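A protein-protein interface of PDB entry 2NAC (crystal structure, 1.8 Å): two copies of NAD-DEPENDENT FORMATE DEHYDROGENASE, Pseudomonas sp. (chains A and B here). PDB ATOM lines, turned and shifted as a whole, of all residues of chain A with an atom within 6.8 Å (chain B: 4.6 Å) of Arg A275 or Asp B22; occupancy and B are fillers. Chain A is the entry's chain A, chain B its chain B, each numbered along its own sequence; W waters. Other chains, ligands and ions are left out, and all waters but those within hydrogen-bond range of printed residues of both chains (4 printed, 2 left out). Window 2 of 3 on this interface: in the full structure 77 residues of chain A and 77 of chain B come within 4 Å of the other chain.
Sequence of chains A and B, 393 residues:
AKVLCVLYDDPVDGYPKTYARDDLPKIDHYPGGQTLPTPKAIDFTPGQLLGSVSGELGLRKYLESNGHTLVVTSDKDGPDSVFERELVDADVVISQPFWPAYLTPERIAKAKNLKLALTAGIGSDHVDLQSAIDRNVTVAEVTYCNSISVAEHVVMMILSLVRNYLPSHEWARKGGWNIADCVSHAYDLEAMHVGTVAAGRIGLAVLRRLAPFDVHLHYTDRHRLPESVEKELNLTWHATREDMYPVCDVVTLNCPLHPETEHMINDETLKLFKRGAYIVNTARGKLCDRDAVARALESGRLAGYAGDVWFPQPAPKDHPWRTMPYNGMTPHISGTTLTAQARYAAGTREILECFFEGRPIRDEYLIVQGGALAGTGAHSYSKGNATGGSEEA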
ATOM      1  N   TYR A 187      12.974  -5.585  -5.686  1.00  0.00           N
ATOM      2  CA  TYR A 187      12.108  -4.670  -5.043  1.00  0.00           C
ATOM      3  C   TYR A 187      12.285  -3.218  -5.546  1.00  0.00           C
ATOM      4  O   TYR A 187      13.262  -2.935  -6.202  1.00  0.00           O
ATOM      5  CB  TYR A 187      12.236  -4.670  -3.514  1.00  0.00           C
ATOM      6  CG  TYR A 187      12.115  -6.042  -2.892  1.00  0.00           C
ATOM      7  CD1 TYR A 187      13.215  -6.852  -2.714  1.00  0.00           C
ATOM      8  CD2 TYR A 187      10.873  -6.515  -2.510  1.00  0.00           C
ATOM      9  CE1 TYR A 187      13.076  -8.136  -2.209  1.00  0.00           C
ATOM     10  CE2 TYR A 187      10.740  -7.776  -1.945  1.00  0.00           C
ATOM     11  CZ  TYR A 187      11.834  -8.560  -1.802  1.00  0.00           C
ATOM     12  OH  TYR A 187      11.751  -9.816  -1.323  1.00  0.00           O
ATOM     13  N   ASP A 249      16.192  -0.434   6.267  1.00  0.00           N
ATOM     14  CA  ASP A 249      16.182  -1.384   5.130  1.00  0.00           C
ATOM     15  C   ASP A 249      17.548  -1.433   4.447  1.00  0.00           C
ATOM     16  O   ASP A 249      18.090  -2.423   3.964  1.00  0.00           O
ATOM     17  CB  ASP A 249      15.092  -1.067   4.096  1.00  0.00           C
ATOM     18  CG  ASP A 249      13.695  -1.255   4.690  1.00  0.00           C
ATOM     19  OD1 ASP A 249      13.463  -2.400   5.124  1.00  0.00           O
ATOM     20  OD2 ASP A 249      13.051  -0.229   4.791  1.00  0.00           O
ATOM     21  N   PHE A 273      20.214  -6.260  12.503  1.00  0.00           N
ATOM     22  CA  PHE A 273      19.661  -5.791  11.229  1.00  0.00           C
ATOM     23  C   PHE A 273      18.418  -6.577  10.876  1.00  0.00           C
ATOM     24  O   PHE A 273      18.286  -7.747  11.210  1.00  0.00           O
ATOM     25  CB  PHE A 273      20.646  -6.021  10.097  1.00  0.00           C
ATOM     26  CG  PHE A 273      21.789  -5.043  10.033  1.00  0.00           C
ATOM     27  CD1 PHE A 273      22.763  -5.026  11.011  1.00  0.00           C
ATOM     28  CD2 PHE A 273      21.886  -4.104   9.022  1.00  0.00           C
ATOM     29  CE1 PHE A 273      23.818  -4.118  11.007  1.00  0.00           C
ATOM     30  CE2 PHE A 273      22.941  -3.169   8.968  1.00  0.00           C
ATOM     31  CZ  PHE A 273      23.908  -3.176   9.967  1.00  0.00           C
ATOM     32  N   LYS A 274      17.502  -5.894  10.253  1.00  0.00           N
ATOM     33  CA  LYS A 274      16.244  -6.546   9.815  1.00  0.00           C
ATOM     34  C   LYS A 274      16.627  -7.562   8.746  1.00  0.00           C
ATOM     35  O   LYS A 274      17.596  -7.461   8.030  1.00  0.00           O
ATOM     36  CB  LYS A 274      15.403  -5.429   9.267  1.00  0.00           C
ATOM     37  CG  LYS A 274      14.396  -5.201   8.215  1.00  0.00           C
ATOM     38  CD  LYS A 274      13.722  -3.817   8.450  1.00  0.00           C
ATOM     39  CE  LYS A 274      12.528  -3.751   7.530  1.00  0.00           C
ATOM     40  NZ  LYS A 274      11.927  -2.415   7.523  1.00  0.00           N
ATOM     41  N   ARG A 275      15.772  -8.615   8.646  1.00  0.00           N
ATOM     42  CA  ARG A 275      15.925  -9.668   7.635  1.00  0.00           C
ATOM     43  C   ARG A 275      15.801  -8.951   6.272  1.00  0.00           C
ATOM     44  O   ARG A 275      14.881  -8.134   6.080  1.00  0.00           O
ATOM     45  CB  ARG A 275      14.713 -10.658   7.702  1.00  0.00           C
ATOM     46  CG  ARG A 275      14.832 -11.777   6.674  1.00  0.00           C
ATOM     47  CD  ARG A 275      13.589 -12.750   6.690  1.00  0.00           C
ATOM     48  NE  ARG A 275      13.735 -13.646   5.526  1.00  0.00           N
ATOM     49  CZ  ARG A 275      14.751 -14.510   5.433  1.00  0.00           C
ATOM     50  NH1 ARG A 275      15.679 -14.626   6.422  1.00  0.00           N
ATOM     51  NH2 ARG A 275      14.918 -15.310   4.383  1.00  0.00           N
ATOM     52  N   GLY A 276      16.754  -9.208   5.423  1.00  0.00           N
ATOM     53  CA  GLY A 276      16.731  -8.628   4.097  1.00  0.00           C
ATOM     54  C   GLY A 276      17.240  -7.217   3.983  1.00  0.00           C
ATOM     55  O   GLY A 276      17.007  -6.519   3.017  1.00  0.00           O
ATOM     56  N   ALA A 277      18.016  -6.775   4.979  1.00  0.00           N
ATOM     57  CA  ALA A 277      18.578  -5.415   4.827  1.00  0.00           C
ATOM     58  C   ALA A 277      19.689  -5.483   3.823  1.00  0.00           C
ATOM     59  O   ALA A 277      20.257  -6.481   3.408  1.00  0.00           O
ATOM     60  CB  ALA A 277      19.234  -5.169   6.184  1.00  0.00           C
ATOM     61  N   SER A 299      23.358 -17.118   4.266  1.00  0.00           N
ATOM     62  CA  SER A 299      22.316 -17.543   5.128  1.00  0.00           C
ATOM     63  C   SER A 299      21.009 -16.828   4.882  1.00  0.00           C
ATOM     64  O   SER A 299      20.010 -17.066   5.546  1.00  0.00           O
ATOM     65  CB  SER A 299      22.810 -17.404   6.575  1.00  0.00           C
ATOM     66  OG  SER A 299      22.711 -16.074   6.959  1.00  0.00           O
ATOM     67  N   GLY A 300      20.933 -15.895   3.924  1.00  0.00           N
ATOM     68  CA  GLY A 300      19.775 -15.132   3.585  1.00  0.00           C
ATOM     69  C   GLY A 300      19.371 -14.062   4.536  1.00  0.00           C
ATOM     70  O   GLY A 300      18.236 -13.583   4.476  1.00  0.00           O
ATOM     71  N   ARG A 301      20.212 -13.602   5.476  1.00  0.00           N
ATOM     72  CA  ARG A 301      19.816 -12.592   6.454  1.00  0.00           C
ATOM     73  C   ARG A 301      19.915 -11.216   5.848  1.00  0.00           C
ATOM     74  O   ARG A 301      19.086 -10.382   6.097  1.00  0.00           O
ATOM     75  CB  ARG A 301      20.661 -12.751   7.710  1.00  0.00           C
ATOM     76  CG  ARG A 301      20.142 -13.942   8.547  1.00  0.00           C
ATOM     77  CD  ARG A 301      19.105 -13.568   9.614  1.00  0.00           C
ATOM     78  NE  ARG A 301      19.574 -12.403  10.345  1.00  0.00           N
ATOM     79  CZ  ARG A 301      19.008 -11.285  10.718  1.00  0.00           C
ATOM     80  NH1 ARG A 301      17.739 -11.027  10.472  1.00  0.00           N
ATOM     81  NH2 ARG A 301      19.743 -10.349  11.291  1.00  0.00           N
ATOM     82  N   LEU A 302      20.951 -11.070   5.045  1.00  0.00           N
ATOM     83  CA  LEU A 302      21.228  -9.870   4.312  1.00  0.00           C
ATOM     84  C   LEU A 302      20.786 -10.149   2.823  1.00  0.00           C
ATOM     85  O   LEU A 302      21.128 -11.152   2.270  1.00  0.00           O
ATOM     86  CB  LEU A 302      22.699  -9.469   4.316  1.00  0.00           C
ATOM     87  CG  LEU A 302      23.441  -8.654   5.362  1.00  0.00           C
ATOM     88  CD1 LEU A 302      24.835  -8.304   4.855  1.00  0.00           C
ATOM     89  CD2 LEU A 302      22.647  -7.444   5.725  1.00  0.00           C
ATOM     90  N   ALA A 303      20.185  -9.190   2.170  1.00  0.00           N
ATOM     91  CA  ALA A 303      19.745  -9.242   0.794  1.00  0.00           C
ATOM     92  C   ALA A 303      20.684  -8.701  -0.242  1.00  0.00           C
ATOM     93  O   ALA A 303      20.574  -8.916  -1.463  1.00  0.00           O
ATOM     94  CB  ALA A 303      18.377  -8.559   0.735  1.00  0.00           C
ATOM     95  N   TYR B  19      11.386 -15.762   0.813  1.00  0.00           N
ATOM     96  CA  TYR B  19      11.672 -14.469   0.203  1.00  0.00           C
ATOM     97  C   TYR B  19      12.734 -13.724   1.051  1.00  0.00           C
ATOM     98  O   TYR B  19      12.901 -14.063   2.218  1.00  0.00           O
ATOM     99  CB  TYR B  19      10.408 -13.641   0.063  1.00  0.00           C
ATOM    100  CG  TYR B  19       9.458 -14.262  -0.952  1.00  0.00           C
ATOM    101  CD1 TYR B  19       9.563 -13.981  -2.295  1.00  0.00           C
ATOM    102  CD2 TYR B  19       8.525 -15.186  -0.484  1.00  0.00           C
ATOM    103  CE1 TYR B  19       8.712 -14.597  -3.212  1.00  0.00           C
ATOM    104  CE2 TYR B  19       7.651 -15.790  -1.393  1.00  0.00           C
ATOM    105  CZ  TYR B  19       7.762 -15.506  -2.724  1.00  0.00           C
ATOM    106  OH  TYR B  19       6.912 -16.154  -3.600  1.00  0.00           O
ATOM    107  N   ALA B  20      13.322 -12.719   0.414  1.00  0.00           N
ATOM    108  CA  ALA B  20      14.399 -11.933   1.124  1.00  0.00           C
ATOM    109  C   ALA B  20      13.900 -11.144   2.275  1.00  0.00           C
ATOM    110  O   ALA B  20      14.703 -10.872   3.190  1.00  0.00           O
ATOM    111  CB  ALA B  20      15.075 -11.077   0.052  1.00  0.00           C
ATOM    112  N   ARG B  21      12.671 -10.695   2.384  1.00  0.00           N
ATOM    113  CA  ARG B  21      12.134  -9.908   3.414  1.00  0.00           C
ATOM    114  C   ARG B  21      10.735 -10.265   3.845  1.00  0.00           C
ATOM    115  O   ARG B  21      10.097 -10.977   3.088  1.00  0.00           O
ATOM    116  CB  ARG B  21      12.207  -8.418   3.099  1.00  0.00           C
ATOM    117  CG  ARG B  21      11.614  -8.080   1.798  1.00  0.00           C
ATOM    118  CD  ARG B  21      11.756  -6.673   1.300  1.00  0.00           C
ATOM    119  NE  ARG B  21      11.385  -5.629   2.181  1.00  0.00           N
ATOM    120  CZ  ARG B  21      12.312  -4.843   2.820  1.00  0.00           C
ATOM    121  NH1 ARG B  21      13.568  -5.036   2.609  1.00  0.00           N
ATOM    122  NH2 ARG B  21      11.719  -3.973   3.592  1.00  0.00           N
ATOM    123  N   ASP B  22      10.346  -9.789   4.983  1.00  0.00           N
ATOM    124  CA  ASP B  22       9.042 -10.124   5.492  1.00  0.00           C
ATOM    125  C   ASP B  22       7.904  -9.276   5.006  1.00  0.00           C
ATOM    126  O   ASP B  22       6.753  -9.760   4.890  1.00  0.00           O
ATOM    127  CB  ASP B  22       9.056 -10.126   7.038  1.00  0.00           C
ATOM    128  CG  ASP B  22       9.949 -11.252   7.516  1.00  0.00           C
ATOM    129  OD1 ASP B  22      10.140 -12.217   6.758  1.00  0.00           O
ATOM    130  OD2 ASP B  22      10.507 -11.109   8.618  1.00  0.00           O
ATOM    131  N   ASP B  23       8.170  -8.019   4.696  1.00  0.00           N
ATOM    132  CA  ASP B  23       7.103  -7.124   4.259  1.00  0.00           C
ATOM    133  C   ASP B  23       7.652  -6.107   3.250  1.00  0.00           C
ATOM    134  O   ASP B  23       8.806  -6.165   2.925  1.00  0.00           O
ATOM    135  CB  ASP B  23       6.471  -6.300   5.413  1.00  0.00           C
ATOM    136  CG  ASP B  23       7.560  -5.649   6.250  1.00  0.00           C
ATOM    137  OD1 ASP B  23       8.552  -5.046   5.764  1.00  0.00           O
ATOM    138  OD2 ASP B  23       7.403  -5.828   7.490  1.00  0.00           O
ATOM    139  N   PRO B  46       1.872  -9.336   0.589  1.00  0.00           N
ATOM    140  CA  PRO B  46       2.690  -8.424  -0.216  1.00  0.00           C
ATOM    141  C   PRO B  46       4.144  -8.848  -0.095  1.00  0.00           C
ATOM    142  O   PRO B  46       4.655  -9.117   0.973  1.00  0.00           O
ATOM    143  CB  PRO B  46       2.393  -7.019   0.298  1.00  0.00           C
ATOM    144  CG  PRO B  46       0.991  -7.239   0.862  1.00  0.00           C
ATOM    145  CD  PRO B  46       1.029  -8.605   1.520  1.00  0.00           C
HETATM  146  O   HOH W   1      17.254 -11.746   2.842  1.00  0.00           O
HETATM  147  O   HOH W   2      15.133  -7.027   0.986  1.00  0.00           O
HETATM  148  O   HOH W   3      12.831 -12.131  -2.361  1.00  0.00           O
HETATM  149  O   HOH W   4      12.122  -8.260   6.682  1.00  0.00           O
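Of the printed residues of chain B, Arg A275 touches Tyr B19, Ala B20 and Asp B22. Printed residues of chain A within 4 Å of Asp B22: Arg A275. Printed residues of chain A within 4 Å of Arg B21: Tyr A187, Asp A249 and Gly A276. Printed residues of chain B within 4 Å of Asp A249: Arg B21 (2.8 Å). Of the printed residues of chain A, Tyr B19 touches Arg A275 (3.2 Å). The nearest printed residue of chain B that does not touch Arg A275 is Arg B21 (4.01 Å). The nearest printed residue of chain A that does not touch Asp B22 is Gly A276 (6.4 Å). The nearest printed residue of chain A that does not touch Arg B21 is Arg A275 (4.01 Å).
Tyr A187 touches Ala B20. OH of Tyr A187 touches CG of Arg B21 (3.6 Å). Ala B20 touches Arg A275. Arg A275 touches Asp B22. Gly A276 touches Arg B21.
No position is printed for both chains. Of the 8 pairs that touch across the chains among the printed residues, none has its exchanged pair printed and touching as well.
Printed residues of chain B that touch a printed residue of chain A: Tyr B19, Ala B20, Arg B21 and Asp B22. Hydrophobic or aromatic side chains of chain B within 4 Å of the printed part of chain A: Ala B20. Hydrophobic or aromatic side chains of chain A that line the printed part of chain B: Tyr A187. Among the printed residues, 8 pairs touch across the chains.
Water W1 bridges the backbone carbonyl oxygen of Gly A300 and the backbone carbonyl oxygen of Ala B20. Water W3 bridges OH of Tyr A187 (2.8 Å) and N of Ala B20 (2.9 Å). Water W2 bridges O of Gly A276 (2.8 Å) and NH1 of Arg B21 (3.0 Å). Water W4 lies within hydrogen-bond range of the backbone carbonyl oxygen (O) of Arg A275 (2.8 Å) and the backbone NH (N) of Asp B22 (2.9 Å).
OD1 of Asp B23 is in salt-bridge range of NH2 of Arg B21 (3.99 Å). The side-chain carboxylate (OD1) of Asp A249 is in salt-bridge range of the side-chain amino group (NZ) of Lys A274, 2.8 Å away. N of Gly A276 sits at hydrogen-bond distance from O of Arg A301. NH1 of Arg A275 sits at hydrogen-bond distance from O of Gly A300.
The backbone NH of Gly A276 lies close to the backbone carbonyl oxygen of Ala B20. The guanidinium group (NH2) of Arg A275 sits at hydrogen-bond distance from the backbone carbonyl oxygen (O) of Tyr B19 (3.2 Å). The side-chain carboxylate (OD1) of Asp A249 lies within salt-bridge range of the guanidinium group (NH2) of Arg B21 (2.8 Å).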
